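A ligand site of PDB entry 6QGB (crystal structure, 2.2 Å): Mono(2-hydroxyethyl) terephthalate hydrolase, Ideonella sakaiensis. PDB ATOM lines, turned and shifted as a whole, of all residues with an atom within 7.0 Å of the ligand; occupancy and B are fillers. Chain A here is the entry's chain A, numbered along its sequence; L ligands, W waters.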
ATOM      1  N   SER A 124      -8.709 -34.963   2.817  1.00  0.00           N
ATOM      2  CA  SER A 124      -7.632 -34.025   2.541  1.00  0.00           C
ATOM      3  C   SER A 124      -8.222 -32.635   2.386  1.00  0.00           C
ATOM      4  O   SER A 124      -9.408 -32.479   2.080  1.00  0.00           O
ATOM      5  CB  SER A 124      -6.860 -34.407   1.274  1.00  0.00           C
ATOM      6  OG  SER A 124      -7.721 -34.399   0.168  1.00  0.00           O
ATOM      7  N   GLY A 125      -7.388 -31.639   2.610  1.00  0.00           N
ATOM      8  CA  GLY A 125      -7.836 -30.262   2.487  1.00  0.00           C
ATOM      9  C   GLY A 125      -8.989 -29.983   3.412  1.00  0.00           C
ATOM     10  O   GLY A 125      -8.979 -30.333   4.592  1.00  0.00           O
ATOM     11  N   THR A 126     -10.028 -29.345   2.878  1.00  0.00           N
ATOM     12  CA  THR A 126     -11.279 -29.161   3.591  1.00  0.00           C
ATOM     13  C   THR A 126     -12.312 -30.195   3.192  1.00  0.00           C
ATOM     14  O   THR A 126     -13.507 -29.967   3.379  1.00  0.00           O
ATOM     15  CB  THR A 126     -11.827 -27.756   3.382  1.00  0.00           C
ATOM     16  OG1 THR A 126     -11.929 -27.494   1.985  1.00  0.00           O
ATOM     17  CG2 THR A 126     -10.931 -26.720   4.036  1.00  0.00           C
ATOM     18  N   ASN A 127     -11.859 -31.322   2.653  1.00  0.00           N
ATOM     19  CA  ASN A 127     -12.728 -32.404   2.160  1.00  0.00           C
ATOM     20  C   ASN A 127     -13.684 -31.831   1.108  1.00  0.00           C
ATOM     21  O   ASN A 127     -13.348 -30.873   0.403  1.00  0.00           O
ATOM     22  CB  ASN A 127     -13.395 -33.098   3.330  1.00  0.00           C
ATOM     23  CG  ASN A 127     -12.462 -34.047   4.060  1.00  0.00           C
ATOM     24  OD1 ASN A 127     -11.452 -34.473   3.517  1.00  0.00           O
ATOM     25  ND2 ASN A 127     -12.793 -34.379   5.286  1.00  0.00           N
ATOM     26  N   CYS A 217      -3.804 -39.082   5.779  1.00  0.00           N
ATOM     27  CA  CYS A 217      -2.731 -38.118   5.937  1.00  0.00           C
ATOM     28  C   CYS A 217      -3.313 -36.726   5.858  1.00  0.00           C
ATOM     29  O   CYS A 217      -4.341 -36.510   5.217  1.00  0.00           O
ATOM     30  CB  CYS A 217      -1.631 -38.289   4.864  1.00  0.00           C
ATOM     31  SG  CYS A 217      -0.108 -37.344   5.218  1.00  0.00           S
ATOM     32  N   SER A 218      -2.665 -35.780   6.545  1.00  0.00           N
ATOM     33  CA  SER A 218      -3.085 -34.385   6.566  1.00  0.00           C
ATOM     34  C   SER A 218      -4.420 -34.253   7.292  1.00  0.00           C
ATOM     35  O   SER A 218      -4.518 -34.624   8.457  1.00  0.00           O
ATOM     36  CB  SER A 218      -3.158 -33.841   5.134  1.00  0.00           C
ATOM     37  OG  SER A 218      -3.485 -32.478   5.142  1.00  0.00           O
ATOM     38  N   GLU A 219      -5.441 -33.734   6.614  1.00  0.00           N
ATOM     39  CA  GLU A 219      -6.785 -33.787   7.177  1.00  0.00           C
ATOM     40  C   GLU A 219      -7.197 -35.240   7.460  1.00  0.00           C
ATOM     41  O   GLU A 219      -7.841 -35.515   8.478  1.00  0.00           O
ATOM     42  CB  GLU A 219      -7.777 -33.104   6.234  1.00  0.00           C
ATOM     43  CG  GLU A 219      -9.214 -33.579   6.369  1.00  0.00           C
ATOM     44  CD  GLU A 219      -9.814 -33.279   7.737  1.00  0.00           C
ATOM     45  OE1 GLU A 219      -9.357 -32.330   8.399  1.00  0.00           O
ATOM     46  OE2 GLU A 219     -10.744 -33.979   8.145  1.00  0.00           O
ATOM     47  N   ALA A 242       1.043 -36.832   8.981  1.00  0.00           N
ATOM     48  CA  ALA A 242       1.066 -35.377   9.130  1.00  0.00           C
ATOM     49  C   ALA A 242      -0.274 -34.863   9.661  1.00  0.00           C
ATOM     50  O   ALA A 242      -0.961 -34.100   8.978  1.00  0.00           O
ATOM     51  CB  ALA A 242       1.410 -34.729   7.790  1.00  0.00           C
ATOM     52  N   LEU A 247      -5.981 -28.354  13.812  1.00  0.00           N
ATOM     53  CA  LEU A 247      -6.193 -27.628  12.564  1.00  0.00           C
ATOM     54  C   LEU A 247      -6.793 -26.229  12.749  1.00  0.00           C
ATOM     55  O   LEU A 247      -6.446 -25.329  11.976  1.00  0.00           O
ATOM     56  CB  LEU A 247      -7.093 -28.449  11.632  1.00  0.00           C
ATOM     57  CG  LEU A 247      -6.445 -28.829  10.298  1.00  0.00           C
ATOM     58  CD1 LEU A 247      -7.200 -29.977   9.665  1.00  0.00           C
ATOM     59  CD2 LEU A 247      -6.378 -27.627   9.343  1.00  0.00           C
ATOM     60  N   ALA A 250      -4.137 -23.532  12.633  1.00  0.00           N
ATOM     61  CA  ALA A 250      -3.300 -23.306  11.467  1.00  0.00           C
ATOM     62  C   ALA A 250      -3.393 -21.853  11.002  1.00  0.00           C
ATOM     63  O   ALA A 250      -2.372 -21.218  10.722  1.00  0.00           O
ATOM     64  CB  ALA A 250      -3.694 -24.259  10.346  1.00  0.00           C
ATOM     65  N   GLY A 251      -4.615 -21.325  10.913  1.00  0.00           N
ATOM     66  CA  GLY A 251      -4.784 -19.942  10.490  1.00  0.00           C
ATOM     67  C   GLY A 251      -4.095 -18.968  11.415  1.00  0.00           C
ATOM     68  O   GLY A 251      -3.661 -17.895  10.992  1.00  0.00           O
ATOM     69  N   TRP A 390       3.353 -22.892   1.223  1.00  0.00           N
ATOM     70  CA  TRP A 390       2.466 -22.757   2.363  1.00  0.00           C
ATOM     71  C   TRP A 390       2.492 -21.347   2.941  1.00  0.00           C
ATOM     72  O   TRP A 390       1.437 -20.718   3.097  1.00  0.00           O
ATOM     73  CB  TRP A 390       2.811 -23.798   3.420  1.00  0.00           C
ATOM     74  CG  TRP A 390       2.380 -25.161   2.996  1.00  0.00           C
ATOM     75  CD1 TRP A 390       3.167 -26.135   2.472  1.00  0.00           C
ATOM     76  CD2 TRP A 390       1.056 -25.699   3.035  1.00  0.00           C
ATOM     77  NE1 TRP A 390       2.426 -27.246   2.182  1.00  0.00           N
ATOM     78  CE2 TRP A 390       1.124 -27.003   2.530  1.00  0.00           C
ATOM     79  CE3 TRP A 390      -0.174 -25.205   3.464  1.00  0.00           C
ATOM     80  CZ2 TRP A 390       0.000 -27.817   2.433  1.00  0.00           C
ATOM     81  CZ3 TRP A 390      -1.284 -26.018   3.362  1.00  0.00           C
ATOM     82  CH2 TRP A 390      -1.191 -27.310   2.844  1.00  0.00           C
ATOM     83  N   GLN A 403      -0.696 -20.567   0.625  1.00  0.00           N
ATOM     84  CA  GLN A 403      -1.831 -21.205   1.269  1.00  0.00           C
ATOM     85  C   GLN A 403      -2.293 -20.426   2.481  1.00  0.00           C
ATOM     86  O   GLN A 403      -3.496 -20.310   2.733  1.00  0.00           O
ATOM     87  CB  GLN A 403      -1.463 -22.634   1.666  1.00  0.00           C
ATOM     88  CG  GLN A 403      -2.128 -23.694   0.842  1.00  0.00           C
ATOM     89  CD  GLN A 403      -1.729 -23.649  -0.614  1.00  0.00           C
ATOM     90  OE1 GLN A 403      -2.534 -23.329  -1.469  1.00  0.00           O
ATOM     91  NE2 GLN A 403      -0.472 -23.985  -0.894  1.00  0.00           N
ATOM     92  N   ARG A 404      -1.354 -19.859   3.234  1.00  0.00           N
ATOM     93  CA  ARG A 404      -1.666 -19.208   4.495  1.00  0.00           C
ATOM     94  C   ARG A 404      -1.840 -17.704   4.382  1.00  0.00           C
ATOM     95  O   ARG A 404      -2.234 -17.071   5.368  1.00  0.00           O
ATOM     96  CB  ARG A 404      -0.561 -19.510   5.516  1.00  0.00           C
ATOM     97  CG  ARG A 404      -0.472 -20.963   5.891  1.00  0.00           C
ATOM     98  CD  ARG A 404      -1.373 -21.281   7.061  1.00  0.00           C
ATOM     99  NE  ARG A 404      -1.740 -22.675   7.098  1.00  0.00           N
ATOM    100  CZ  ARG A 404      -0.941 -23.666   7.477  1.00  0.00           C
ATOM    101  NH1 ARG A 404       0.306 -23.410   7.861  1.00  0.00           N
ATOM    102  NH2 ARG A 404      -1.397 -24.905   7.470  1.00  0.00           N
ATOM    103  N   PHE A 408      -6.452 -21.347   0.611  1.00  0.00           N
ATOM    104  CA  PHE A 408      -7.574 -22.019   1.244  1.00  0.00           C
ATOM    105  C   PHE A 408      -7.418 -22.094   2.756  1.00  0.00           C
ATOM    106  O   PHE A 408      -8.421 -22.128   3.473  1.00  0.00           O
ATOM    107  CB  PHE A 408      -7.760 -23.418   0.651  1.00  0.00           C
ATOM    108  CG  PHE A 408      -6.900 -24.480   1.283  1.00  0.00           C
ATOM    109  CD1 PHE A 408      -5.620 -24.713   0.835  1.00  0.00           C
ATOM    110  CD2 PHE A 408      -7.394 -25.265   2.308  1.00  0.00           C
ATOM    111  CE1 PHE A 408      -4.847 -25.699   1.400  1.00  0.00           C
ATOM    112  CE2 PHE A 408      -6.618 -26.247   2.882  1.00  0.00           C
ATOM    113  CZ  PHE A 408      -5.351 -26.464   2.419  1.00  0.00           C
ATOM    114  N   SER A 409      -6.191 -22.133   3.258  1.00  0.00           N
ATOM    115  CA  SER A 409      -5.995 -22.231   4.701  1.00  0.00           C
ATOM    116  C   SER A 409      -6.499 -20.975   5.401  1.00  0.00           C
ATOM    117  O   SER A 409      -7.262 -21.054   6.375  1.00  0.00           O
ATOM    118  CB  SER A 409      -4.534 -22.476   5.036  1.00  0.00           C
ATOM    119  OG  SER A 409      -4.362 -22.639   6.424  1.00  0.00           O
ATOM    120  N   ALA A 410      -6.084 -19.806   4.917  1.00  0.00           N
ATOM    121  CA  ALA A 410      -6.610 -18.561   5.469  1.00  0.00           C
ATOM    122  C   ALA A 410      -8.117 -18.481   5.292  1.00  0.00           C
ATOM    123  O   ALA A 410      -8.838 -18.091   6.210  1.00  0.00           O
ATOM    124  CB  ALA A 410      -5.918 -17.373   4.828  1.00  0.00           C
ATOM    125  N   SER A 412     -10.202 -21.008   5.107  1.00  0.00           N
ATOM    126  CA  SER A 412     -10.845 -21.990   5.969  1.00  0.00           C
ATOM    127  C   SER A 412     -10.937 -21.494   7.396  1.00  0.00           C
ATOM    128  O   SER A 412     -11.954 -21.676   8.059  1.00  0.00           O
ATOM    129  CB  SER A 412     -10.099 -23.325   5.907  1.00  0.00           C
ATOM    130  OG  SER A 412     -10.758 -24.302   6.692  1.00  0.00           O
ATOM    131  N   TRP A 413      -9.877 -20.857   7.888  1.00  0.00           N
ATOM    132  CA  TRP A 413      -9.924 -20.331   9.243  1.00  0.00           C
ATOM    133  C   TRP A 413     -11.038 -19.320   9.390  1.00  0.00           C
ATOM    134  O   TRP A 413     -11.745 -19.310  10.411  1.00  0.00           O
ATOM    135  CB  TRP A 413      -8.585 -19.715   9.629  1.00  0.00           C
ATOM    136  CG  TRP A 413      -8.509 -19.469  11.087  1.00  0.00           C
ATOM    137  CD1 TRP A 413      -8.040 -20.327  12.024  1.00  0.00           C
ATOM    138  CD2 TRP A 413      -8.943 -18.301  11.794  1.00  0.00           C
ATOM    139  NE1 TRP A 413      -8.143 -19.770  13.266  1.00  0.00           N
ATOM    140  CE2 TRP A 413      -8.689 -18.526  13.154  1.00  0.00           C
ATOM    141  CE3 TRP A 413      -9.518 -17.089  11.409  1.00  0.00           C
ATOM    142  CZ2 TRP A 413      -9.000 -17.590  14.136  1.00  0.00           C
ATOM    143  CZ3 TRP A 413      -9.810 -16.162  12.379  1.00  0.00           C
ATOM    144  CH2 TRP A 413      -9.553 -16.416  13.727  1.00  0.00           C
ATOM    145  N   PHE A 417     -13.501 -22.131  10.969  1.00  0.00           N
ATOM    146  CA  PHE A 417     -12.975 -22.299  12.303  1.00  0.00           C
ATOM    147  C   PHE A 417     -13.270 -21.129  13.230  1.00  0.00           C
ATOM    148  O   PHE A 417     -13.465 -21.347  14.422  1.00  0.00           O
ATOM    149  CB  PHE A 417     -11.462 -22.539  12.244  1.00  0.00           C
ATOM    150  CG  PHE A 417     -11.094 -23.776  11.485  1.00  0.00           C
ATOM    151  CD1 PHE A 417     -11.872 -24.907  11.568  1.00  0.00           C
ATOM    152  CD2 PHE A 417      -9.965 -23.803  10.691  1.00  0.00           C
ATOM    153  CE1 PHE A 417     -11.537 -26.051  10.877  1.00  0.00           C
ATOM    154  CE2 PHE A 417      -9.625 -24.941   9.996  1.00  0.00           C
ATOM    155  CZ  PHE A 417     -10.407 -26.061  10.087  1.00  0.00           C
ATOM    156  N   ASP A 485       7.468 -30.222   6.824  1.00  0.00           N
ATOM    157  CA  ASP A 485       6.053 -29.940   6.619  1.00  0.00           C
ATOM    158  C   ASP A 485       5.758 -28.517   7.113  1.00  0.00           C
ATOM    159  O   ASP A 485       5.970 -28.202   8.283  1.00  0.00           O
ATOM    160  CB  ASP A 485       5.231 -30.975   7.375  1.00  0.00           C
ATOM    161  CG  ASP A 485       3.743 -30.897   7.091  1.00  0.00           C
ATOM    162  OD1 ASP A 485       3.212 -29.805   6.850  1.00  0.00           O
ATOM    163  OD2 ASP A 485       3.093 -31.956   7.138  1.00  0.00           O
ATOM    164  N   ALA A 487       2.624 -27.204   6.563  1.00  0.00           N
ATOM    165  CA  ALA A 487       1.201 -27.141   6.891  1.00  0.00           C
ATOM    166  C   ALA A 487       0.974 -27.381   8.375  1.00  0.00           C
ATOM    167  O   ALA A 487       0.352 -26.569   9.050  1.00  0.00           O
ATOM    168  CB  ALA A 487       0.428 -28.158   6.057  1.00  0.00           C
ATOM    169  N   PHE A 488       1.491 -28.493   8.890  1.00  0.00           N
ATOM    170  CA  PHE A 488       1.446 -28.805  10.308  1.00  0.00           C
ATOM    171  C   PHE A 488       2.853 -29.100  10.783  1.00  0.00           C
ATOM    172  O   PHE A 488       3.642 -29.731  10.079  1.00  0.00           O
ATOM    173  CB  PHE A 488       0.519 -29.985  10.582  1.00  0.00           C
ATOM    174  CG  PHE A 488      -0.815 -29.857   9.923  1.00  0.00           C
ATOM    175  CD1 PHE A 488      -1.641 -28.796  10.225  1.00  0.00           C
ATOM    176  CD2 PHE A 488      -1.242 -30.783   8.991  1.00  0.00           C
ATOM    177  CE1 PHE A 488      -2.867 -28.658   9.610  1.00  0.00           C
ATOM    178  CE2 PHE A 488      -2.452 -30.658   8.377  1.00  0.00           C
ATOM    179  CZ  PHE A 488      -3.276 -29.592   8.688  1.00  0.00           C
ATOM    180  N   HIS A 521       4.771 -31.911   3.161  1.00  0.00           N
ATOM    181  CA  HIS A 521       3.474 -32.283   3.719  1.00  0.00           C
ATOM    182  C   HIS A 521       2.949 -33.536   3.034  1.00  0.00           C
ATOM    183  O   HIS A 521       2.603 -33.512   1.850  1.00  0.00           O
ATOM    184  CB  HIS A 521       2.487 -31.132   3.584  1.00  0.00           C
ATOM    185  CG  HIS A 521       1.152 -31.387   4.215  1.00  0.00           C
ATOM    186  ND1 HIS A 521       1.009 -31.927   5.469  1.00  0.00           N
ATOM    187  CD2 HIS A 521      -0.098 -31.183   3.747  1.00  0.00           C
ATOM    188  CE1 HIS A 521      -0.269 -32.039   5.756  1.00  0.00           C
ATOM    189  NE2 HIS A 521      -0.965 -31.589   4.730  1.00  0.00           N
HETATM  190  C1  LIG L   1      -5.271 -25.884   6.555  1.00  0.00           C
HETATM  191  O1  LIG L   1      -6.457 -25.536   6.729  1.00  0.00           O
HETATM  192  O2  LIG L   1      -4.349 -25.105   6.840  1.00  0.00           O
HETATM  193  C2  LIG L   1      -4.959 -27.215   5.979  1.00  0.00           C
HETATM  194  C3  LIG L   1      -5.986 -28.114   5.756  1.00  0.00           C
HETATM  195  C4  LIG L   1      -5.720 -29.358   5.200  1.00  0.00           C
HETATM  196  C5  LIG L   1      -4.419 -29.693   4.871  1.00  0.00           C
HETATM  197  C6  LIG L   1      -3.386 -28.805   5.086  1.00  0.00           C
HETATM  198  C7  LIG L   1      -3.652 -27.560   5.642  1.00  0.00           C
HETATM  199  O   HOH W   1      -8.808 -26.482   6.890  1.00  0.00           O
HETATM  200  O   HOH W   2      -7.175 -23.242   8.121  1.00  0.00           O
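Water W1 lies within hydrogen-bond range of an oxygen (O1) of the ligand and the side-chain hydroxyl (OG) of Ser 412. Water W2 lies within hydrogen-bond range of an oxygen (O1) of the ligand (2.8 Å) and the backbone carbonyl oxygen of Ser 409 (2.8 Å).
An oxygen (O2) of the ligand lies within hydrogen-bond range of the side-chain hydroxyl (OG) of Ser 409 (2.5 Å). NH2 of Arg 404 lies within salt-bridge range of O2 of the ligand, at 3.0 Å.
Residues that only touch the ligand: Gly 125 (3.5 Å), Ser 218 (2.9 Å), Leu 247 (3.3 Å), Ala 250 (3.7 Å), Trp 390 (3.5 Å), Phe 408 (3.5 Å), Ala 487 (3.99 Å), Phe 488 (3.7 Å) and His 521 (3.7 Å). Of the 24 residues printed, 11 come within 4 Å of the ligand. The nearest printed residue that does not touch the ligand is Ser 412 (4.3 Å).
OG of Ser 409 lies within hydrogen-bond range of NE of Arg 404. O of Gln 403 lies within hydrogen-bond range of N of Ser 409, 3.3 Å away. NE2 of His 521 lies within hydrogen-bond range of OG of Ser 218 (2.7 Å). N of Ser 218 sits close to O of Ala 242 (3.4 Å). O of Trp 390 lies within hydrogen-bond range of N of Arg 404 (2.9 Å). The guanidinium group (NH2) of Arg 404 lies within hydrogen-bond range of the backbone carbonyl oxygen (O) of Ala 487 (2.9 Å). N of Phe 488 lies within hydrogen-bond range of OD1 of Asp 485 (3.0 Å). ND1 of His 521 is in hydrogen-bond range of OD2 of Asp 485 (2.7 Å).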
